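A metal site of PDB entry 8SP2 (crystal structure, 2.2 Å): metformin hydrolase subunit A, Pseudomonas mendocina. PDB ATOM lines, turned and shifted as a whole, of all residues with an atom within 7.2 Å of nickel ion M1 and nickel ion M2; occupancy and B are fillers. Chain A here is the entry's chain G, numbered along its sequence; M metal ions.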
ATOM      1  N   ASP A 158     -25.473  -8.061   3.201  1.00  0.00           N
ATOM      2  CA  ASP A 158     -24.147  -8.592   2.913  1.00  0.00           C
ATOM      3  C   ASP A 158     -24.213  -9.756   1.907  1.00  0.00           C
ATOM      4  O   ASP A 158     -25.286 -10.224   1.514  1.00  0.00           O
ATOM      5  CB  ASP A 158     -23.430  -8.996   4.201  1.00  0.00           C
ATOM      6  CG  ASP A 158     -24.079 -10.171   4.915  1.00  0.00           C
ATOM      7  OD1 ASP A 158     -24.334 -11.165   4.229  1.00  0.00           O
ATOM      8  OD2 ASP A 158     -24.292 -10.090   6.149  1.00  0.00           O
ATOM      9  N   HIS A 159     -23.034 -10.231   1.491  1.00  0.00           N
ATOM     10  CA  HIS A 159     -22.956 -11.207   0.419  1.00  0.00           C
ATOM     11  C   HIS A 159     -23.167 -12.641   0.896  1.00  0.00           C
ATOM     12  O   HIS A 159     -22.848 -13.558   0.155  1.00  0.00           O
ATOM     13  CB  HIS A 159     -21.596 -11.159  -0.282  1.00  0.00           C
ATOM     14  CG  HIS A 159     -21.728 -11.525  -1.720  1.00  0.00           C
ATOM     15  ND1 HIS A 159     -20.701 -11.373  -2.618  1.00  0.00           N
ATOM     16  CD2 HIS A 159     -22.779 -11.936  -2.409  1.00  0.00           C
ATOM     17  CE1 HIS A 159     -21.148 -11.726  -3.818  1.00  0.00           C
ATOM     18  NE2 HIS A 159     -22.409 -12.070  -3.720  1.00  0.00           N
ATOM     19  N   SER A 160     -23.712 -12.839   2.110  1.00  0.00           N
ATOM     20  CA  SER A 160     -24.245 -14.141   2.485  1.00  0.00           C
ATOM     21  C   SER A 160     -25.502 -14.417   1.661  1.00  0.00           C
ATOM     22  O   SER A 160     -25.937 -15.570   1.553  1.00  0.00           O
ATOM     23  CB  SER A 160     -24.517 -14.243   3.975  1.00  0.00           C
ATOM     24  OG  SER A 160     -25.639 -13.461   4.365  1.00  0.00           O
ATOM     25  N   PRO A 162     -26.440 -14.897  -1.486  1.00  0.00           N
ATOM     26  CA  PRO A 162     -26.515 -16.034  -2.420  1.00  0.00           C
ATOM     27  C   PRO A 162     -26.632 -17.444  -1.814  1.00  0.00           C
ATOM     28  O   PRO A 162     -27.044 -18.390  -2.502  1.00  0.00           O
ATOM     29  CB  PRO A 162     -25.223 -15.947  -3.250  1.00  0.00           C
ATOM     30  CG  PRO A 162     -24.297 -15.032  -2.483  1.00  0.00           C
ATOM     31  CD  PRO A 162     -25.215 -14.119  -1.696  1.00  0.00           C
ATOM     32  N   HIS A 182     -21.324 -15.271 -10.447  1.00  0.00           N
ATOM     33  CA  HIS A 182     -20.878 -14.469  -9.322  1.00  0.00           C
ATOM     34  C   HIS A 182     -19.979 -13.338  -9.799  1.00  0.00           C
ATOM     35  O   HIS A 182     -18.849 -13.576 -10.213  1.00  0.00           O
ATOM     36  CB  HIS A 182     -20.099 -15.363  -8.347  1.00  0.00           C
ATOM     37  CG  HIS A 182     -19.838 -14.789  -6.989  1.00  0.00           C
ATOM     38  ND1 HIS A 182     -20.553 -15.192  -5.883  1.00  0.00           N
ATOM     39  CD2 HIS A 182     -18.953 -13.885  -6.552  1.00  0.00           C
ATOM     40  CE1 HIS A 182     -20.108 -14.536  -4.814  1.00  0.00           C
ATOM     41  NE2 HIS A 182     -19.133 -13.753  -5.193  1.00  0.00           N
ATOM     42  N   VAL A 183     -20.455 -12.093  -9.701  1.00  0.00           N
ATOM     43  CA  VAL A 183     -19.678 -10.955 -10.181  1.00  0.00           C
ATOM     44  C   VAL A 183     -19.280 -10.117  -8.966  1.00  0.00           C
ATOM     45  O   VAL A 183     -20.139  -9.645  -8.230  1.00  0.00           O
ATOM     46  CB  VAL A 183     -20.449 -10.137 -11.224  1.00  0.00           C
ATOM     47  CG1 VAL A 183     -19.705  -8.858 -11.618  1.00  0.00           C
ATOM     48  CG2 VAL A 183     -20.765 -10.959 -12.457  1.00  0.00           C
ATOM     49  N   ASP A 184     -17.976  -9.944  -8.790  1.00  0.00           N
ATOM     50  CA  ASP A 184     -17.428  -9.533  -7.508  1.00  0.00           C
ATOM     51  C   ASP A 184     -15.939  -9.264  -7.715  1.00  0.00           C
ATOM     52  O   ASP A 184     -15.339  -9.856  -8.592  1.00  0.00           O
ATOM     53  CB  ASP A 184     -17.689 -10.635  -6.483  1.00  0.00           C
ATOM     54  CG  ASP A 184     -17.626 -10.234  -5.016  1.00  0.00           C
ATOM     55  OD1 ASP A 184     -16.987  -9.188  -4.694  1.00  0.00           O
ATOM     56  OD2 ASP A 184     -18.231 -10.971  -4.192  1.00  0.00           O
ATOM     57  N   CYS A 185     -15.398  -8.325  -6.926  1.00  0.00           N
ATOM     58  CA  CYS A 185     -13.972  -8.109  -6.750  1.00  0.00           C
ATOM     59  C   CYS A 185     -13.312  -9.261  -5.987  1.00  0.00           C
ATOM     60  O   CYS A 185     -12.106  -9.513  -6.112  1.00  0.00           O
ATOM     61  CB  CYS A 185     -13.753  -6.861  -5.903  1.00  0.00           C
ATOM     62  SG  CYS A 185     -12.014  -6.398  -5.743  1.00  0.00           S
ATOM     63  N   HIS A 186     -14.108  -9.879  -5.115  1.00  0.00           N
ATOM     64  CA  HIS A 186     -13.668 -10.921  -4.199  1.00  0.00           C
ATOM     65  C   HIS A 186     -14.141 -12.256  -4.749  1.00  0.00           C
ATOM     66  O   HIS A 186     -15.256 -12.382  -5.244  1.00  0.00           O
ATOM     67  CB  HIS A 186     -14.231 -10.661  -2.799  1.00  0.00           C
ATOM     68  CG  HIS A 186     -13.988  -9.271  -2.307  1.00  0.00           C
ATOM     69  ND1 HIS A 186     -14.967  -8.320  -2.059  1.00  0.00           N
ATOM     70  CD2 HIS A 186     -12.813  -8.655  -2.086  1.00  0.00           C
ATOM     71  CE1 HIS A 186     -14.389  -7.204  -1.664  1.00  0.00           C
ATOM     72  NE2 HIS A 186     -13.088  -7.378  -1.676  1.00  0.00           N
ATOM     73  N   LEU A 187     -13.277 -13.266  -4.610  1.00  0.00           N
ATOM     74  CA  LEU A 187     -13.531 -14.584  -5.149  1.00  0.00           C
ATOM     75  C   LEU A 187     -14.596 -15.345  -4.343  1.00  0.00           C
ATOM     76  O   LEU A 187     -15.309 -16.162  -4.916  1.00  0.00           O
ATOM     77  CB  LEU A 187     -12.189 -15.332  -5.204  1.00  0.00           C
ATOM     78  CG  LEU A 187     -11.233 -14.873  -6.307  1.00  0.00           C
ATOM     79  CD1 LEU A 187      -9.893 -15.568  -6.166  1.00  0.00           C
ATOM     80  CD2 LEU A 187     -11.815 -15.138  -7.699  1.00  0.00           C
ATOM     81  N   ASP A 188     -14.712 -15.062  -3.033  1.00  0.00           N
ATOM     82  CA  ASP A 188     -15.785 -15.600  -2.193  1.00  0.00           C
ATOM     83  C   ASP A 188     -15.886 -17.127  -2.300  1.00  0.00           C
ATOM     84  O   ASP A 188     -16.969 -17.663  -2.537  1.00  0.00           O
ATOM     85  CB  ASP A 188     -17.145 -14.982  -2.561  1.00  0.00           C
ATOM     86  CG  ASP A 188     -17.377 -13.549  -2.091  1.00  0.00           C
ATOM     87  OD1 ASP A 188     -16.423 -12.913  -1.645  1.00  0.00           O
ATOM     88  OD2 ASP A 188     -18.544 -13.130  -2.061  1.00  0.00           O
ATOM     89  N   ASN A 200     -20.278 -14.466   4.307  1.00  0.00           N
ATOM     90  CA  ASN A 200     -20.525 -13.793   3.040  1.00  0.00           C
ATOM     91  C   ASN A 200     -19.410 -14.059   2.038  1.00  0.00           C
ATOM     92  O   ASN A 200     -19.511 -13.623   0.897  1.00  0.00           O
ATOM     93  CB  ASN A 200     -20.696 -12.285   3.220  1.00  0.00           C
ATOM     94  CG  ASN A 200     -19.427 -11.550   3.630  1.00  0.00           C
ATOM     95  OD1 ASN A 200     -18.535 -12.094   4.269  1.00  0.00           O
ATOM     96  ND2 ASN A 200     -19.385 -10.265   3.302  1.00  0.00           N
ATOM     97  N   CYS A 201     -18.358 -14.781   2.462  1.00  0.00           N
ATOM     98  CA  CYS A 201     -17.286 -15.100   1.539  1.00  0.00           C
ATOM     99  C   CYS A 201     -17.235 -16.592   1.185  1.00  0.00           C
ATOM    100  O   CYS A 201     -16.158 -17.129   0.936  1.00  0.00           O
ATOM    101  CB  CYS A 201     -15.956 -14.641   2.122  1.00  0.00           C
ATOM    102  SG  CYS A 201     -15.565 -15.472   3.681  1.00  0.00           S
ATOM    103  N   SER A 202     -18.396 -17.233   1.045  1.00  0.00           N
ATOM    104  CA  SER A 202     -18.448 -18.656   0.681  1.00  0.00           C
ATOM    105  C   SER A 202     -19.621 -18.939  -0.253  1.00  0.00           C
ATOM    106  O   SER A 202     -20.066 -20.090  -0.352  1.00  0.00           O
ATOM    107  CB  SER A 202     -18.527 -19.542   1.894  1.00  0.00           C
ATOM    108  OG  SER A 202     -17.331 -19.427   2.648  1.00  0.00           O
ATOM    109  N   HIS A 220     -17.201 -16.940 -12.383  1.00  0.00           N
ATOM    110  CA  HIS A 220     -16.913 -15.742 -11.618  1.00  0.00           C
ATOM    111  C   HIS A 220     -16.343 -14.662 -12.534  1.00  0.00           C
ATOM    112  O   HIS A 220     -15.585 -14.976 -13.443  1.00  0.00           O
ATOM    113  CB  HIS A 220     -15.962 -16.075 -10.465  1.00  0.00           C
ATOM    114  CG  HIS A 220     -15.747 -14.964  -9.489  1.00  0.00           C
ATOM    115  ND1 HIS A 220     -15.102 -13.804  -9.807  1.00  0.00           N
ATOM    116  CD2 HIS A 220     -16.076 -14.865  -8.186  1.00  0.00           C
ATOM    117  CE1 HIS A 220     -15.020 -13.035  -8.727  1.00  0.00           C
ATOM    118  NE2 HIS A 220     -15.620 -13.644  -7.733  1.00  0.00           N
ATOM    119  N   LEU A 227      -7.530  -8.767  -1.500  1.00  0.00           N
ATOM    120  CA  LEU A 227      -8.393  -9.386  -0.505  1.00  0.00           C
ATOM    121  C   LEU A 227      -8.995 -10.643  -1.122  1.00  0.00           C
ATOM    122  O   LEU A 227     -10.191 -10.704  -1.407  1.00  0.00           O
ATOM    123  CB  LEU A 227      -9.484  -8.439  -0.006  1.00  0.00           C
ATOM    124  CG  LEU A 227     -10.272  -8.960   1.208  1.00  0.00           C
ATOM    125  CD1 LEU A 227      -9.614  -8.524   2.513  1.00  0.00           C
ATOM    126  CD2 LEU A 227     -11.728  -8.523   1.166  1.00  0.00           C
ATOM    127  N   TRP A 232      -9.379 -19.302  -2.043  1.00  0.00           N
ATOM    128  CA  TRP A 232     -10.536 -18.869  -2.820  1.00  0.00           C
ATOM    129  C   TRP A 232     -10.231 -19.093  -4.293  1.00  0.00           C
ATOM    130  O   TRP A 232     -11.079 -19.586  -5.018  1.00  0.00           O
ATOM    131  CB  TRP A 232     -10.906 -17.407  -2.548  1.00  0.00           C
ATOM    132  CG  TRP A 232     -11.295 -17.081  -1.141  1.00  0.00           C
ATOM    133  CD1 TRP A 232     -11.269 -17.907  -0.058  1.00  0.00           C
ATOM    134  CD2 TRP A 232     -11.740 -15.801  -0.666  1.00  0.00           C
ATOM    135  NE1 TRP A 232     -11.682 -17.228   1.063  1.00  0.00           N
ATOM    136  CE2 TRP A 232     -11.973 -15.933   0.713  1.00  0.00           C
ATOM    137  CE3 TRP A 232     -11.960 -14.549  -1.268  1.00  0.00           C
ATOM    138  CZ2 TRP A 232     -12.419 -14.863   1.501  1.00  0.00           C
ATOM    139  CZ3 TRP A 232     -12.400 -13.504  -0.497  1.00  0.00           C
ATOM    140  CH2 TRP A 232     -12.636 -13.659   0.873  1.00  0.00           C
ATOM    141  N   THR A 275     -25.584 -13.437  -8.717  1.00  0.00           N
ATOM    142  CA  THR A 275     -25.269 -12.555  -7.605  1.00  0.00           C
ATOM    143  C   THR A 275     -24.226 -11.514  -8.028  1.00  0.00           C
ATOM    144  O   THR A 275     -23.205 -11.860  -8.619  1.00  0.00           O
ATOM    145  CB  THR A 275     -24.747 -13.327  -6.381  1.00  0.00           C
ATOM    146  OG1 THR A 275     -24.547 -12.432  -5.276  1.00  0.00           O
ATOM    147  CG2 THR A 275     -23.453 -14.062  -6.657  1.00  0.00           C
ATOM    148  N   ASP A 277     -22.022  -8.278  -6.590  1.00  0.00           N
ATOM    149  CA  ASP A 277     -21.489  -7.439  -5.529  1.00  0.00           C
ATOM    150  C   ASP A 277     -21.115  -6.058  -6.075  1.00  0.00           C
ATOM    151  O   ASP A 277     -20.385  -5.948  -7.060  1.00  0.00           O
ATOM    152  CB  ASP A 277     -20.269  -8.100  -4.910  1.00  0.00           C
ATOM    153  CG  ASP A 277     -19.906  -7.600  -3.529  1.00  0.00           C
ATOM    154  OD1 ASP A 277     -20.082  -6.380  -3.264  1.00  0.00           O
ATOM    155  OD2 ASP A 277     -19.427  -8.438  -2.710  1.00  0.00           O
ATOM    156  N   THR A 278     -21.584  -5.017  -5.396  1.00  0.00           N
ATOM    157  CA  THR A 278     -21.333  -3.647  -5.838  1.00  0.00           C
ATOM    158  C   THR A 278     -19.853  -3.284  -5.690  1.00  0.00           C
ATOM    159  O   THR A 278     -19.403  -2.276  -6.253  1.00  0.00           O
ATOM    160  CB  THR A 278     -22.277  -2.665  -5.138  1.00  0.00           C
ATOM    161  OG1 THR A 278     -22.190  -2.832  -3.724  1.00  0.00           O
ATOM    162  CG2 THR A 278     -23.718  -2.867  -5.550  1.00  0.00           C
ATOM    163  N   ASP A 279     -19.036  -4.127  -5.037  1.00  0.00           N
ATOM    164  CA  ASP A 279     -17.620  -3.824  -5.093  1.00  0.00           C
ATOM    165  C   ASP A 279     -16.966  -4.377  -6.358  1.00  0.00           C
ATOM    166  O   ASP A 279     -15.755  -4.228  -6.547  1.00  0.00           O
ATOM    167  CB  ASP A 279     -16.869  -4.293  -3.868  1.00  0.00           C
ATOM    168  CG  ASP A 279     -16.993  -5.782  -3.710  1.00  0.00           C
ATOM    169  OD1 ASP A 279     -17.057  -6.477  -4.769  1.00  0.00           O
ATOM    170  OD2 ASP A 279     -17.080  -6.197  -2.542  1.00  0.00           O
ATOM    171  N   SER A 280     -17.735  -4.973  -7.261  1.00  0.00           N
ATOM    172  CA  SER A 280     -17.244  -5.125  -8.633  1.00  0.00           C
ATOM    173  C   SER A 280     -17.066  -3.754  -9.301  1.00  0.00           C
ATOM    174  O   SER A 280     -16.235  -3.590 -10.192  1.00  0.00           O
ATOM    175  CB  SER A 280     -18.150  -6.015  -9.406  1.00  0.00           C
ATOM    176  OG  SER A 280     -19.452  -5.463  -9.557  1.00  0.00           O
ATOM    177  N   ASN A 289     -19.515   1.194  -0.006  1.00  0.00           N
ATOM    178  CA  ASN A 289     -19.387  -0.252  -0.009  1.00  0.00           C
ATOM    179  C   ASN A 289     -18.760  -0.721   1.293  1.00  0.00           C
ATOM    180  O   ASN A 289     -18.051   0.024   1.951  1.00  0.00           O
ATOM    181  CB  ASN A 289     -18.590  -0.727  -1.216  1.00  0.00           C
ATOM    182  CG  ASN A 289     -18.863  -2.171  -1.523  1.00  0.00           C
ATOM    183  OD1 ASN A 289     -18.114  -3.056  -1.098  1.00  0.00           O
ATOM    184  ND2 ASN A 289     -19.945  -2.422  -2.234  1.00  0.00           N
ATOM    185  N   ALA A 291     -16.482  -3.022   1.386  1.00  0.00           N
ATOM    186  CA  ALA A 291     -15.071  -3.227   1.087  1.00  0.00           C
ATOM    187  C   ALA A 291     -14.789  -2.723  -0.315  1.00  0.00           C
ATOM    188  O   ALA A 291     -14.647  -3.517  -1.241  1.00  0.00           O
ATOM    189  CB  ALA A 291     -14.733  -4.689   1.195  1.00  0.00           C
ATOM    190  N   GLU A 293     -13.169  -1.082  -3.792  1.00  0.00           N
ATOM    191  CA  GLU A 293     -11.931  -1.420  -4.475  1.00  0.00           C
ATOM    192  C   GLU A 293     -11.784  -0.605  -5.753  1.00  0.00           C
ATOM    193  O   GLU A 293     -12.709  -0.552  -6.560  1.00  0.00           O
ATOM    194  CB  GLU A 293     -11.961  -2.899  -4.852  1.00  0.00           C
ATOM    195  CG  GLU A 293     -11.887  -3.845  -3.674  1.00  0.00           C
ATOM    196  CD  GLU A 293     -10.477  -4.085  -3.160  1.00  0.00           C
ATOM    197  OE1 GLU A 293      -9.571  -3.246  -3.470  1.00  0.00           O
ATOM    198  OE2 GLU A 293     -10.286  -5.119  -2.480  1.00  0.00           O
ATOM    199  N   VAL A 320     -25.620  -6.915  -3.810  1.00  0.00           N
ATOM    200  CA  VAL A 320     -25.235  -6.910  -2.395  1.00  0.00           C
ATOM    201  C   VAL A 320     -24.205  -5.810  -2.105  1.00  0.00           C
ATOM    202  O   VAL A 320     -23.590  -5.248  -3.019  1.00  0.00           O
ATOM    203  CB  VAL A 320     -24.674  -8.280  -1.943  1.00  0.00           C
ATOM    204  CG1 VAL A 320     -25.625  -9.413  -2.286  1.00  0.00           C
ATOM    205  CG2 VAL A 320     -23.305  -8.562  -2.530  1.00  0.00           C
ATOM    206  N   GLU A 321     -24.062  -5.559  -0.787  1.00  0.00           N
ATOM    207  CA  GLU A 321     -22.977  -4.846  -0.117  1.00  0.00           C
ATOM    208  C   GLU A 321     -23.008  -3.336  -0.356  1.00  0.00           C
ATOM    209  O   GLU A 321     -22.000  -2.689  -0.074  1.00  0.00           O
ATOM    210  CB  GLU A 321     -21.598  -5.441  -0.446  1.00  0.00           C
ATOM    211  CG  GLU A 321     -21.399  -6.901   0.014  1.00  0.00           C
ATOM    212  CD  GLU A 321     -21.142  -7.185   1.501  1.00  0.00           C
ATOM    213  OE1 GLU A 321     -21.171  -6.236   2.311  1.00  0.00           O
ATOM    214  OE2 GLU A 321     -20.928  -8.404   1.858  1.00  0.00           O
HETATM  215 NI    NI M   1     -18.613 -10.849  -2.113  1.00  0.00          NI
HETATM  216 NI    NI M   2     -17.078  -8.364  -2.596  1.00  0.00          NI
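NE2 of His 182 lies close to OD2 of Asp 184 (3.1 Å). OD1 of Asp 279 sits at hydrogen-bond distance from N of Cys 185, 3.3 Å away. N of Asp 279 sits close to ND2 of Asn 289, 3.4 Å away. The backbone carbonyl oxygen of His 186 lies within hydrogen-bond range of a ring nitrogen (NE2) of His 220 (2.8 Å). The side-chain hydroxyl (OG1) of Thr 275 lies within hydrogen-bond range of a ring nitrogen (NE2) of His 159 (2.7 Å). A ring nitrogen (NE2) of His 182 lies close to the side-chain carboxylate (OD2) of Asp 188, at 3.2 Å. O of Asp 277 lies within hydrogen-bond range of OG of Ser 280 (2.7 Å). N of Asp 277 is in hydrogen-bond range of O of Val 183 (2.8 Å).
The nearest printed residue that does not touch nickel ion M1 is Asn 200 (4.2 Å).
Four residues have an atom within 4 Å of nickel ion M2: Asp 184, His 186, Asp 277 and Asp 279. Along chain A the residues within 4 Å of nickel ion M2 span positions 184 to 279.
Nickel ion M1 is bound by OD2 of Asp 184 (2.1 Å), ND1 of His 159 (2.2 Å) and OD2 of Asp 188 (2.3 Å). Slightly farther from nickel ion M1 lies OD2 of Asp 277 (2.6 Å).
Nickel ion M2 is bound by OD2 of Asp 279 (2.2 Å), ND1 of His 186 (2.2 Å), OD1 of Asp 184 (2.3 Å) and OD2 of Asp 277 (2.4 Å). Nickel ion M2 has four donor atoms within binding distance.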
